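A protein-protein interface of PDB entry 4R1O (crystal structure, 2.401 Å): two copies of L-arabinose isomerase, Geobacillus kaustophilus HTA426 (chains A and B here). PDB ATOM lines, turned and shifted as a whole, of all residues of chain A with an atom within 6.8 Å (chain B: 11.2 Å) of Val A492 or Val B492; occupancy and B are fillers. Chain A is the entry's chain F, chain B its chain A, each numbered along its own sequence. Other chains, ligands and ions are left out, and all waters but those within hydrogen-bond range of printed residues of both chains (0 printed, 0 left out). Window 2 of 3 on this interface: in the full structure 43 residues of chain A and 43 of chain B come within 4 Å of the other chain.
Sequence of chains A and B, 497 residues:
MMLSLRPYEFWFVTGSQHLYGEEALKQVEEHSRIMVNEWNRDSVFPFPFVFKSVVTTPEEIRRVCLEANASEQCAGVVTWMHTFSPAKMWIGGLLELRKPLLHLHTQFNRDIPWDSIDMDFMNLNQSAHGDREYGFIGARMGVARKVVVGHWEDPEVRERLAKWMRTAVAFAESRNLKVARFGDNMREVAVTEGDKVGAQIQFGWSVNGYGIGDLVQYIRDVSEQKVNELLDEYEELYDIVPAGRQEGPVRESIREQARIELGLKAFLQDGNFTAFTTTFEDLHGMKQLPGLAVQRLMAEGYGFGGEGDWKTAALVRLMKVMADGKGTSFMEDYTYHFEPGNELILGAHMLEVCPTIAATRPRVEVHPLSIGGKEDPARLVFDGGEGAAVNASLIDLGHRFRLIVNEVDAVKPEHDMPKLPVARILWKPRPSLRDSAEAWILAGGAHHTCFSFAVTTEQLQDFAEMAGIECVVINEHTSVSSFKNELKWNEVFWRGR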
ATOM      1  N   ARG A 400      -8.593  17.188  42.823  1.00  0.00           N
ATOM      2  CA  ARG A 400      -7.417  16.760  42.070  1.00  0.00           C
ATOM      3  C   ARG A 400      -6.515  17.938  41.739  1.00  0.00           C
ATOM      4  O   ARG A 400      -6.879  19.092  41.975  1.00  0.00           O
ATOM      5  CB  ARG A 400      -7.845  16.059  40.776  1.00  0.00           C
ATOM      6  CG  ARG A 400      -8.624  16.952  39.825  1.00  0.00           C
ATOM      7  CD  ARG A 400      -9.216  16.177  38.662  1.00  0.00           C
ATOM      8  NE  ARG A 400      -9.890  17.070  37.720  1.00  0.00           N
ATOM      9  CZ  ARG A 400      -9.250  17.773  36.794  1.00  0.00           C
ATOM     10  NH1 ARG A 400      -7.929  17.666  36.696  1.00  0.00           N
ATOM     11  NH2 ARG A 400      -9.916  18.575  35.971  1.00  0.00           N
ATOM     12  N   LEU A 487     -10.884  21.881  28.928  1.00  0.00           N
ATOM     13  CA  LEU A 487     -11.065  21.926  30.378  1.00  0.00           C
ATOM     14  C   LEU A 487     -12.287  21.127  30.797  1.00  0.00           C
ATOM     15  O   LEU A 487     -12.225  20.366  31.755  1.00  0.00           O
ATOM     16  CB  LEU A 487     -11.178  23.371  30.878  1.00  0.00           C
ATOM     17  CG  LEU A 487      -9.921  24.234  30.734  1.00  0.00           C
ATOM     18  CD1 LEU A 487     -10.177  25.621  31.275  1.00  0.00           C
ATOM     19  CD2 LEU A 487      -8.773  23.584  31.484  1.00  0.00           C
ATOM     20  N   LYS A 488     -13.384  21.284  30.061  1.00  0.00           N
ATOM     21  CA  LYS A 488     -14.622  20.575  30.366  1.00  0.00           C
ATOM     22  C   LYS A 488     -14.459  19.089  30.174  1.00  0.00           C
ATOM     23  O   LYS A 488     -14.804  18.299  31.046  1.00  0.00           O
ATOM     24  CB  LYS A 488     -15.768  21.060  29.475  1.00  0.00           C
ATOM     25  CG  LYS A 488     -16.339  22.390  29.902  1.00  0.00           C
ATOM     26  CD  LYS A 488     -17.290  22.992  28.871  1.00  0.00           C
ATOM     27  CE  LYS A 488     -18.021  24.189  29.482  1.00  0.00           C
ATOM     28  NZ  LYS A 488     -18.295  25.275  28.497  1.00  0.00           N
ATOM     29  N   TRP A 489     -13.961  18.704  29.008  1.00  0.00           N
ATOM     30  CA  TRP A 489     -13.878  17.291  28.654  1.00  0.00           C
ATOM     31  C   TRP A 489     -12.847  16.574  29.527  1.00  0.00           C
ATOM     32  O   TRP A 489     -13.088  15.459  29.986  1.00  0.00           O
ATOM     33  CB  TRP A 489     -13.564  17.132  27.165  1.00  0.00           C
ATOM     34  CG  TRP A 489     -14.582  17.769  26.258  1.00  0.00           C
ATOM     35  CD1 TRP A 489     -15.916  17.958  26.517  1.00  0.00           C
ATOM     36  CD2 TRP A 489     -14.350  18.302  24.943  1.00  0.00           C
ATOM     37  NE1 TRP A 489     -16.528  18.558  25.438  1.00  0.00           N
ATOM     38  CE2 TRP A 489     -15.588  18.786  24.462  1.00  0.00           C
ATOM     39  CE3 TRP A 489     -13.222  18.393  24.117  1.00  0.00           C
ATOM     40  CZ2 TRP A 489     -15.724  19.372  23.194  1.00  0.00           C
ATOM     41  CZ3 TRP A 489     -13.355  18.981  22.854  1.00  0.00           C
ATOM     42  CH2 TRP A 489     -14.603  19.457  22.406  1.00  0.00           C
ATOM     43  N   ASN A 490     -11.714  17.230  29.777  1.00  0.00           N
ATOM     44  CA  ASN A 490     -10.738  16.717  30.737  1.00  0.00           C
ATOM     45  C   ASN A 490     -11.350  16.527  32.126  1.00  0.00           C
ATOM     46  O   ASN A 490     -11.105  15.504  32.773  1.00  0.00           O
ATOM     47  CB  ASN A 490      -9.524  17.652  30.826  1.00  0.00           C
ATOM     48  CG  ASN A 490      -8.624  17.556  29.613  1.00  0.00           C
ATOM     49  OD1 ASN A 490      -8.868  16.764  28.704  1.00  0.00           O
ATOM     50  ND2 ASN A 490      -7.586  18.374  29.583  1.00  0.00           N
ATOM     51  N   GLU A 491     -12.128  17.525  32.564  1.00  0.00           N
ATOM     52  CA  GLU A 491     -12.867  17.524  33.831  1.00  0.00           C
ATOM     53  C   GLU A 491     -13.501  16.190  34.143  1.00  0.00           C
ATOM     54  O   GLU A 491     -13.241  15.615  35.189  1.00  0.00           O
ATOM     55  CB  GLU A 491     -14.004  18.582  33.793  1.00  0.00           C
ATOM     56  CG  GLU A 491     -14.371  19.263  35.132  1.00  0.00           C
ATOM     57  CD  GLU A 491     -15.566  18.631  35.864  1.00  0.00           C
ATOM     58  OE1 GLU A 491     -16.158  17.642  35.352  1.00  0.00           O
ATOM     59  OE2 GLU A 491     -15.911  19.138  36.965  1.00  0.00           O
ATOM     60  N   VAL A 492     -14.365  15.715  33.249  1.00  0.00           N
ATOM     61  CA  VAL A 492     -15.101  14.489  33.533  1.00  0.00           C
ATOM     62  C   VAL A 492     -14.204  13.284  33.440  1.00  0.00           C
ATOM     63  O   VAL A 492     -14.399  12.325  34.169  1.00  0.00           O
ATOM     64  CB  VAL A 492     -16.373  14.284  32.658  1.00  0.00           C
ATOM     65  CG1 VAL A 492     -17.593  14.857  33.355  1.00  0.00           C
ATOM     66  CG2 VAL A 492     -16.217  14.878  31.299  1.00  0.00           C
ATOM     67  N   PHE A 493     -13.213  13.329  32.556  1.00  0.00           N
ATOM     68  CA  PHE A 493     -12.252  12.242  32.505  1.00  0.00           C
ATOM     69  C   PHE A 493     -11.517  12.063  33.824  1.00  0.00           C
ATOM     70  O   PHE A 493     -11.402  10.948  34.312  1.00  0.00           O
ATOM     71  CB  PHE A 493     -11.237  12.401  31.378  1.00  0.00           C
ATOM     72  CG  PHE A 493     -10.146  11.361  31.422  1.00  0.00           C
ATOM     73  CD1 PHE A 493     -10.411  10.049  31.068  1.00  0.00           C
ATOM     74  CD2 PHE A 493      -8.869  11.690  31.835  1.00  0.00           C
ATOM     75  CE1 PHE A 493      -9.427   9.077  31.116  1.00  0.00           C
ATOM     76  CE2 PHE A 493      -7.855  10.720  31.876  1.00  0.00           C
ATOM     77  CZ  PHE A 493      -8.141   9.409  31.517  1.00  0.00           C
ATOM     78  N   TRP A 494     -11.034  13.157  34.411  1.00  0.00           N
ATOM     79  CA  TRP A 494     -10.189  13.043  35.603  1.00  0.00           C
ATOM     80  C   TRP A 494     -10.941  12.827  36.927  1.00  0.00           C
ATOM     81  O   TRP A 494     -10.324  12.432  37.911  1.00  0.00           O
ATOM     82  CB  TRP A 494      -9.179  14.201  35.713  1.00  0.00           C
ATOM     83  CG  TRP A 494      -8.061  14.124  34.705  1.00  0.00           C
ATOM     84  CD1 TRP A 494      -7.948  14.848  33.549  1.00  0.00           C
ATOM     85  CD2 TRP A 494      -6.916  13.264  34.749  1.00  0.00           C
ATOM     86  NE1 TRP A 494      -6.813  14.491  32.876  1.00  0.00           N
ATOM     87  CE2 TRP A 494      -6.158  13.522  33.589  1.00  0.00           C
ATOM     88  CE3 TRP A 494      -6.462  12.291  35.652  1.00  0.00           C
ATOM     89  CZ2 TRP A 494      -4.962  12.844  33.309  1.00  0.00           C
ATOM     90  CZ3 TRP A 494      -5.280  11.624  35.381  1.00  0.00           C
ATOM     91  CH2 TRP A 494      -4.540  11.903  34.219  1.00  0.00           C
ATOM     92  N   ARG A 495     -12.256  13.043  36.957  1.00  0.00           N
ATOM     93  CA  ARG A 495     -13.004  12.884  38.216  1.00  0.00           C
ATOM     94  C   ARG A 495     -12.892  11.481  38.785  1.00  0.00           C
ATOM     95  O   ARG A 495     -12.973  10.497  38.049  1.00  0.00           O
ATOM     96  CB  ARG A 495     -14.481  13.242  38.053  1.00  0.00           C
ATOM     97  CG  ARG A 495     -14.719  14.689  37.660  1.00  0.00           C
ATOM     98  CD  ARG A 495     -16.013  15.242  38.224  1.00  0.00           C
ATOM     99  NE  ARG A 495     -15.902  15.537  39.652  1.00  0.00           N
ATOM    100  CZ  ARG A 495     -15.735  16.759  40.148  1.00  0.00           C
ATOM    101  NH1 ARG A 495     -15.650  16.940  41.467  1.00  0.00           N
ATOM    102  NH2 ARG A 495     -15.658  17.802  39.324  1.00  0.00           N
ATOM    103  N   GLY A 496     -12.693  11.392  40.096  1.00  0.00           N
ATOM    104  CA  GLY A 496     -12.666  10.105  40.771  1.00  0.00           C
ATOM    105  C   GLY A 496     -11.267   9.600  41.074  1.00  0.00           C
ATOM    106  O   GLY A 496     -10.467   9.358  40.166  1.00  0.00           O
ATOM    107  N   LEU B 397     -11.650  -4.251  25.742  1.00  0.00           N
ATOM    108  CA  LEU B 397     -11.096  -3.522  26.881  1.00  0.00           C
ATOM    109  C   LEU B 397     -11.606  -4.036  28.229  1.00  0.00           C
ATOM    110  O   LEU B 397     -11.337  -3.432  29.267  1.00  0.00           O
ATOM    111  CB  LEU B 397     -11.445  -2.037  26.764  1.00  0.00           C
ATOM    112  CG  LEU B 397     -10.797  -1.274  25.617  1.00  0.00           C
ATOM    113  CD1 LEU B 397     -11.333   0.148  25.544  1.00  0.00           C
ATOM    114  CD2 LEU B 397      -9.276  -1.285  25.761  1.00  0.00           C
ATOM    115  N   HIS B 399     -14.622  -4.084  29.608  1.00  0.00           N
ATOM    116  CA  HIS B 399     -15.998  -3.653  29.843  1.00  0.00           C
ATOM    117  C   HIS B 399     -16.712  -3.260  28.544  1.00  0.00           C
ATOM    118  O   HIS B 399     -17.921  -3.076  28.527  1.00  0.00           O
ATOM    119  CB  HIS B 399     -16.044  -2.505  30.861  1.00  0.00           C
ATOM    120  CG  HIS B 399     -15.256  -1.301  30.445  1.00  0.00           C
ATOM    121  ND1 HIS B 399     -13.882  -1.316  30.323  1.00  0.00           N
ATOM    122  CD2 HIS B 399     -15.647  -0.047  30.118  1.00  0.00           C
ATOM    123  CE1 HIS B 399     -13.461  -0.124  29.940  1.00  0.00           C
ATOM    124  NE2 HIS B 399     -14.511   0.666  29.812  1.00  0.00           N
ATOM    125  N   ARG B 400     -15.962  -3.129  27.460  1.00  0.00           N
ATOM    126  CA  ARG B 400     -16.544  -2.759  26.168  1.00  0.00           C
ATOM    127  C   ARG B 400     -15.568  -3.075  25.039  1.00  0.00           C
ATOM    128  O   ARG B 400     -14.411  -3.405  25.282  1.00  0.00           O
ATOM    129  CB  ARG B 400     -16.923  -1.268  26.136  1.00  0.00           C
ATOM    130  CG  ARG B 400     -15.736  -0.325  26.358  1.00  0.00           C
ATOM    131  CD  ARG B 400     -16.181   1.120  26.380  1.00  0.00           C
ATOM    132  NE  ARG B 400     -15.060   2.041  26.549  1.00  0.00           N
ATOM    133  CZ  ARG B 400     -14.381   2.572  25.536  1.00  0.00           C
ATOM    134  NH1 ARG B 400     -14.716   2.283  24.290  1.00  0.00           N
ATOM    135  NH2 ARG B 400     -13.366   3.397  25.764  1.00  0.00           N
ATOM    136  N   ARG B 402     -13.663  -1.881  21.296  1.00  0.00           N
ATOM    137  CA  ARG B 402     -13.168  -0.705  20.581  1.00  0.00           C
ATOM    138  C   ARG B 402     -12.691  -1.131  19.203  1.00  0.00           C
ATOM    139  O   ARG B 402     -11.907  -2.061  19.082  1.00  0.00           O
ATOM    140  CB  ARG B 402     -12.006  -0.054  21.336  1.00  0.00           C
ATOM    141  CG  ARG B 402     -11.250   0.976  20.506  1.00  0.00           C
ATOM    142  CD  ARG B 402      -9.992   1.521  21.212  1.00  0.00           C
ATOM    143  NE  ARG B 402     -10.305   2.347  22.375  1.00  0.00           N
ATOM    144  CZ  ARG B 402      -9.503   2.490  23.426  1.00  0.00           C
ATOM    145  NH1 ARG B 402      -8.327   1.869  23.475  1.00  0.00           N
ATOM    146  NH2 ARG B 402      -9.885   3.255  24.435  1.00  0.00           N
ATOM    147  N   GLU B 470     -17.267   2.148  20.279  1.00  0.00           N
ATOM    148  CA  GLU B 470     -16.330   3.194  19.939  1.00  0.00           C
ATOM    149  C   GLU B 470     -15.550   2.761  18.709  1.00  0.00           C
ATOM    150  O   GLU B 470     -15.170   1.590  18.600  1.00  0.00           O
ATOM    151  CB  GLU B 470     -15.363   3.426  21.107  1.00  0.00           C
ATOM    152  CG  GLU B 470     -14.308   4.490  20.831  1.00  0.00           C
ATOM    153  CD  GLU B 470     -13.113   4.429  21.773  1.00  0.00           C
ATOM    154  OE1 GLU B 470     -12.938   3.421  22.502  1.00  0.00           O
ATOM    155  OE2 GLU B 470     -12.346   5.409  21.776  1.00  0.00           O
ATOM    156  N   VAL B 472     -12.163   4.348  16.455  1.00  0.00           N
ATOM    157  CA  VAL B 472     -11.131   5.364  16.285  1.00  0.00           C
ATOM    158  C   VAL B 472     -10.392   5.134  14.970  1.00  0.00           C
ATOM    159  O   VAL B 472     -10.197   3.989  14.543  1.00  0.00           O
ATOM    160  CB  VAL B 472     -10.156   5.388  17.473  1.00  0.00           C
ATOM    161  CG1 VAL B 472     -10.844   5.981  18.692  1.00  0.00           C
ATOM    162  CG2 VAL B 472      -9.683   3.984  17.794  1.00  0.00           C
ATOM    163  N   LYS B 484      -4.621  10.973  21.391  1.00  0.00           N
ATOM    164  CA  LYS B 484      -4.545  10.600  22.791  1.00  0.00           C
ATOM    165  C   LYS B 484      -5.733  11.170  23.571  1.00  0.00           C
ATOM    166  O   LYS B 484      -6.327  10.472  24.395  1.00  0.00           O
ATOM    167  CB  LYS B 484      -3.228  11.078  23.385  1.00  0.00           C
ATOM    168  CG  LYS B 484      -2.864  10.374  24.664  1.00  0.00           C
ATOM    169  CD  LYS B 484      -1.419  10.651  25.060  1.00  0.00           C
ATOM    170  CE  LYS B 484      -1.110   9.966  26.374  1.00  0.00           C
ATOM    171  NZ  LYS B 484      -2.228  10.186  27.347  1.00  0.00           N
ATOM    172  N   ASN B 485      -6.089  12.425  23.297  1.00  0.00           N
ATOM    173  CA  ASN B 485      -7.221  13.051  23.968  1.00  0.00           C
ATOM    174  C   ASN B 485      -8.551  12.410  23.596  1.00  0.00           C
ATOM    175  O   ASN B 485      -9.406  12.242  24.448  1.00  0.00           O
ATOM    176  CB  ASN B 485      -7.274  14.552  23.693  1.00  0.00           C
ATOM    177  CG  ASN B 485      -6.169  15.307  24.395  1.00  0.00           C
ATOM    178  OD1 ASN B 485      -5.597  14.816  25.360  1.00  0.00           O
ATOM    179  ND2 ASN B 485      -5.865  16.502  23.914  1.00  0.00           N
ATOM    180  N   GLU B 486      -8.724  12.057  22.327  1.00  0.00           N
ATOM    181  CA  GLU B 486      -9.969  11.444  21.884  1.00  0.00           C
ATOM    182  C   GLU B 486     -10.263  10.180  22.680  1.00  0.00           C
ATOM    183  O   GLU B 486     -11.409   9.931  23.034  1.00  0.00           O
ATOM    184  CB  GLU B 486      -9.932  11.080  20.408  1.00  0.00           C
ATOM    185  CG  GLU B 486     -10.071  12.223  19.441  1.00  0.00           C
ATOM    186  CD  GLU B 486     -10.310  11.718  18.017  1.00  0.00           C
ATOM    187  OE1 GLU B 486     -10.094  12.509  17.068  1.00  0.00           O
ATOM    188  OE2 GLU B 486     -10.719  10.532  17.854  1.00  0.00           O
ATOM    189  N   LEU B 487      -9.230   9.385  22.951  1.00  0.00           N
ATOM    190  CA  LEU B 487      -9.417   8.109  23.623  1.00  0.00           C
ATOM    191  C   LEU B 487      -9.881   8.355  25.042  1.00  0.00           C
ATOM    192  O   LEU B 487     -10.743   7.639  25.561  1.00  0.00           O
ATOM    193  CB  LEU B 487      -8.129   7.300  23.647  1.00  0.00           C
ATOM    194  CG  LEU B 487      -7.514   6.783  22.353  1.00  0.00           C
ATOM    195  CD1 LEU B 487      -6.118   6.251  22.655  1.00  0.00           C
ATOM    196  CD2 LEU B 487      -8.390   5.707  21.709  1.00  0.00           C
ATOM    197  N   LYS B 488      -9.301   9.373  25.665  1.00  0.00           N
ATOM    198  CA  LYS B 488      -9.689   9.768  27.005  1.00  0.00           C
ATOM    199  C   LYS B 488     -11.143  10.221  27.019  1.00  0.00           C
ATOM    200  O   LYS B 488     -11.964   9.712  27.786  1.00  0.00           O
ATOM    201  CB  LYS B 488      -8.787  10.901  27.517  1.00  0.00           C
ATOM    202  CG  LYS B 488      -7.439  10.442  28.064  1.00  0.00           C
ATOM    203  CD  LYS B 488      -6.528  11.627  28.430  1.00  0.00           C
ATOM    204  CE  LYS B 488      -5.304  11.166  29.216  1.00  0.00           C
ATOM    205  NZ  LYS B 488      -4.148  12.101  29.068  1.00  0.00           N
ATOM    206  N   TRP B 489     -11.457  11.198  26.179  1.00  0.00           N
ATOM    207  CA  TRP B 489     -12.802  11.750  26.153  1.00  0.00           C
ATOM    208  C   TRP B 489     -13.850  10.680  25.749  1.00  0.00           C
ATOM    209  O   TRP B 489     -14.902  10.583  26.384  1.00  0.00           O
ATOM    210  CB  TRP B 489     -12.841  12.979  25.249  1.00  0.00           C
ATOM    211  CG  TRP B 489     -11.887  14.062  25.685  1.00  0.00           C
ATOM    212  CD1 TRP B 489     -11.466  14.321  26.956  1.00  0.00           C
ATOM    213  CD2 TRP B 489     -11.237  15.024  24.846  1.00  0.00           C
ATOM    214  NE1 TRP B 489     -10.617  15.393  26.967  1.00  0.00           N
ATOM    215  CE2 TRP B 489     -10.443  15.835  25.682  1.00  0.00           C
ATOM    216  CE3 TRP B 489     -11.245  15.276  23.465  1.00  0.00           C
ATOM    217  CZ2 TRP B 489      -9.663  16.882  25.191  1.00  0.00           C
ATOM    218  CZ3 TRP B 489     -10.465  16.322  22.970  1.00  0.00           C
ATOM    219  CH2 TRP B 489      -9.692  17.116  23.839  1.00  0.00           C
ATOM    220  N   ASN B 490     -13.542   9.866  24.735  1.00  0.00           N
ATOM    221  CA  ASN B 490     -14.368   8.710  24.379  1.00  0.00           C
ATOM    222  C   ASN B 490     -14.617   7.745  25.553  1.00  0.00           C
ATOM    223  O   ASN B 490     -15.745   7.302  25.766  1.00  0.00           O
ATOM    224  CB  ASN B 490     -13.757   7.939  23.204  1.00  0.00           C
ATOM    225  CG  ASN B 490     -13.849   8.694  21.880  1.00  0.00           C
ATOM    226  OD1 ASN B 490     -14.406   9.789  21.809  1.00  0.00           O
ATOM    227  ND2 ASN B 490     -13.277   8.117  20.828  1.00  0.00           N
ATOM    228  N   GLU B 491     -13.538   7.419  26.270  1.00  0.00           N
ATOM    229  CA  GLU B 491     -13.527   6.617  27.497  1.00  0.00           C
ATOM    230  C   GLU B 491     -14.681   6.967  28.436  1.00  0.00           C
ATOM    231  O   GLU B 491     -15.467   6.101  28.816  1.00  0.00           O
ATOM    232  CB  GLU B 491     -12.184   6.866  28.234  1.00  0.00           C
ATOM    233  CG  GLU B 491     -11.635   5.795  29.204  1.00  0.00           C
ATOM    234  CD  GLU B 491     -12.355   5.737  30.552  1.00  0.00           C
ATOM    235  OE1 GLU B 491     -12.561   6.803  31.185  1.00  0.00           O
ATOM    236  OE2 GLU B 491     -12.708   4.612  30.983  1.00  0.00           O
ATOM    237  N   VAL B 492     -14.778   8.235  28.821  1.00  0.00           N
ATOM    238  CA  VAL B 492     -15.843   8.642  29.718  1.00  0.00           C
ATOM    239  C   VAL B 492     -17.210   8.462  29.068  1.00  0.00           C
ATOM    240  O   VAL B 492     -18.176   8.137  29.743  1.00  0.00           O
ATOM    241  CB  VAL B 492     -15.741  10.119  30.147  1.00  0.00           C
ATOM    242  CG1 VAL B 492     -16.441  10.305  31.481  1.00  0.00           C
ATOM    243  CG2 VAL B 492     -14.316  10.549  30.244  1.00  0.00           C
ATOM    244  N   PHE B 493     -17.290   8.694  27.763  1.00  0.00           N
ATOM    245  CA  PHE B 493     -18.568   8.644  27.078  1.00  0.00           C
ATOM    246  C   PHE B 493     -19.126   7.225  26.940  1.00  0.00           C
ATOM    247  O   PHE B 493     -20.324   7.010  27.101  1.00  0.00           O
ATOM    248  CB  PHE B 493     -18.487   9.301  25.694  1.00  0.00           C
ATOM    249  CG  PHE B 493     -19.704   9.052  24.866  1.00  0.00           C
ATOM    250  CD1 PHE B 493     -20.867   9.766  25.101  1.00  0.00           C
ATOM    251  CD2 PHE B 493     -19.710   8.072  23.893  1.00  0.00           C
ATOM    252  CE1 PHE B 493     -22.013   9.519  24.365  1.00  0.00           C
ATOM    253  CE2 PHE B 493     -20.864   7.811  23.158  1.00  0.00           C
ATOM    254  CZ  PHE B 493     -22.008   8.543  23.390  1.00  0.00           C
ATOM    255  N   TRP B 494     -18.254   6.268  26.620  1.00  0.00           N
ATOM    256  CA  TRP B 494     -18.666   4.890  26.352  1.00  0.00           C
ATOM    257  C   TRP B 494     -18.817   4.002  27.593  1.00  0.00           C
ATOM    258  O   TRP B 494     -19.336   2.888  27.501  1.00  0.00           O
ATOM    259  CB  TRP B 494     -17.704   4.237  25.369  1.00  0.00           C
ATOM    260  CG  TRP B 494     -17.913   4.699  23.991  1.00  0.00           C
ATOM    261  CD1 TRP B 494     -17.097   5.516  23.269  1.00  0.00           C
ATOM    262  CD2 TRP B 494     -19.031   4.401  23.153  1.00  0.00           C
ATOM    263  NE1 TRP B 494     -17.640   5.744  22.035  1.00  0.00           N
ATOM    264  CE2 TRP B 494     -18.825   5.067  21.934  1.00  0.00           C
ATOM    265  CE3 TRP B 494     -20.189   3.631  23.316  1.00  0.00           C
ATOM    266  CZ2 TRP B 494     -19.726   4.985  20.875  1.00  0.00           C
ATOM    267  CZ3 TRP B 494     -21.086   3.550  22.264  1.00  0.00           C
ATOM    268  CH2 TRP B 494     -20.846   4.221  21.057  1.00  0.00           C
ATOM    269  N   ARG B 495     -18.363   4.491  28.743  1.00  0.00           N
ATOM    270  CA  ARG B 495     -18.477   3.737  29.987  1.00  0.00           C
ATOM    271  C   ARG B 495     -19.934   3.513  30.396  1.00  0.00           C
ATOM    272  O   ARG B 495     -20.708   4.462  30.528  1.00  0.00           O
ATOM    273  CB  ARG B 495     -17.716   4.429  31.117  1.00  0.00           C
ATOM    274  CG  ARG B 495     -18.144   3.947  32.498  1.00  0.00           C
ATOM    275  CD  ARG B 495     -17.016   3.979  33.511  1.00  0.00           C
ATOM    276  NE  ARG B 495     -16.032   2.911  33.311  1.00  0.00           N
ATOM    277  CZ  ARG B 495     -14.850   3.085  32.722  1.00  0.00           C
ATOM    278  NH1 ARG B 495     -14.509   4.285  32.262  1.00  0.00           N
ATOM    279  NH2 ARG B 495     -14.010   2.062  32.592  1.00  0.00           N
ATOM    280  N   GLY B 496     -20.302   2.250  30.595  1.00  0.00           N
ATOM    281  CA  GLY B 496     -21.660   1.891  30.972  1.00  0.00           C
ATOM    282  C   GLY B 496     -22.609   1.877  29.781  1.00  0.00           C
ATOM    283  O   GLY B 496     -23.608   1.153  29.769  1.00  0.00           O
ATOM    284  N   ARG B 497     -22.280   2.675  28.769  1.00  0.00           N
ATOM    285  CA  ARG B 497     -23.134   2.847  27.599  1.00  0.00           C
ATOM    286  C   ARG B 497     -23.149   1.608  26.705  1.00  0.00           C
ATOM    287  O   ARG B 497     -24.162   0.910  26.605  1.00  0.00           O
ATOM    288  CB  ARG B 497     -22.687   4.077  26.805  1.00  0.00           C
ATOM    289  CG  ARG B 497     -23.467   4.313  25.534  1.00  0.00           C
ATOM    290  CD  ARG B 497     -23.042   5.620  24.876  1.00  0.00           C
ATOM    291  NE  ARG B 497     -23.306   6.775  25.734  1.00  0.00           N
ATOM    292  CZ  ARG B 497     -24.437   7.477  25.714  1.00  0.00           C
ATOM    293  NH1 ARG B 497     -24.593   8.510  26.530  1.00  0.00           N
ATOM    294  NH2 ARG B 497     -25.412   7.150  24.876  1.00  0.00           N
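NE1 of Trp B489 is in hydrogen-bond range of OD1 of Asn A490 (2.8 Å).
The side-chain carboxylate (OE2) of Glu B491 is in salt-bridge range of the guanidinium group (NH2) of Arg B495.
Trp A489 touches Trp B489 (CB to NE1, 3.4 Å). Val B492 touches Val A492. CD1 of Phe A493 touches O of Lys B488 (3.6 Å). Phe A493 touches Glu B491. Val B492 touches Phe A493 (CG2 to CA, 3.5 Å).
Val A492 touches one residue of chain B. Of chain A, only Val A492 (3.9 Å) and Phe A493 (3.5 Å) come within 4 Å of Val B492. No residue of chain B comes within 4 Å of Glu A491. Of the printed residues of chain A, Lys B488 touches Phe A493. Of the printed residues of chain A, Trp B489 touches Trp A489 (3.4 Å) and Asn A490 (2.8 Å). Leu B487 touches none of the printed residues of chain A. Arg B497 touches none of the printed residues of chain A. The nearest printed residue of chain B that does not touch Trp A489 is Val B492 (5.1 Å).
Hydrophobic or aromatic side chains of chain B that line the printed part of chain A: Trp B489 and Val B492. Of the 11 printed residues of chain A, 4 touch a printed residue of chain B. Printed residues of chain A that touch a printed residue of chain B: Trp A489, Asn A490, Val A492 and Phe A493. Hydrophobic or aromatic side chains of chain A that line the printed part of chain B: Trp A489 and Phe A493.
Asn A490 touches Trp B489, but with the chains exchanged Trp A489 does not touch Asn B490 (7.7 Å). Phe A493 touches Lys B488, but with the chains exchanged Lys A488 does not touch Phe B493 (10.5 Å). Phe A493 touches Glu B491, but with the chains exchanged Glu A491 does not touch Phe B493 (10.5 Å). Phe A493 touches Val B492, but with the chains exchanged Val A492 does not touch Phe B493 (7.2 Å). Positions printed for both chains: 400, 487, 488, 489, 490, 491, 492, 493, 494, 495 and 496. Of the 6 pairs that touch across the chains among the printed residues, 2 have their exchanged pair printed and touching as well.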
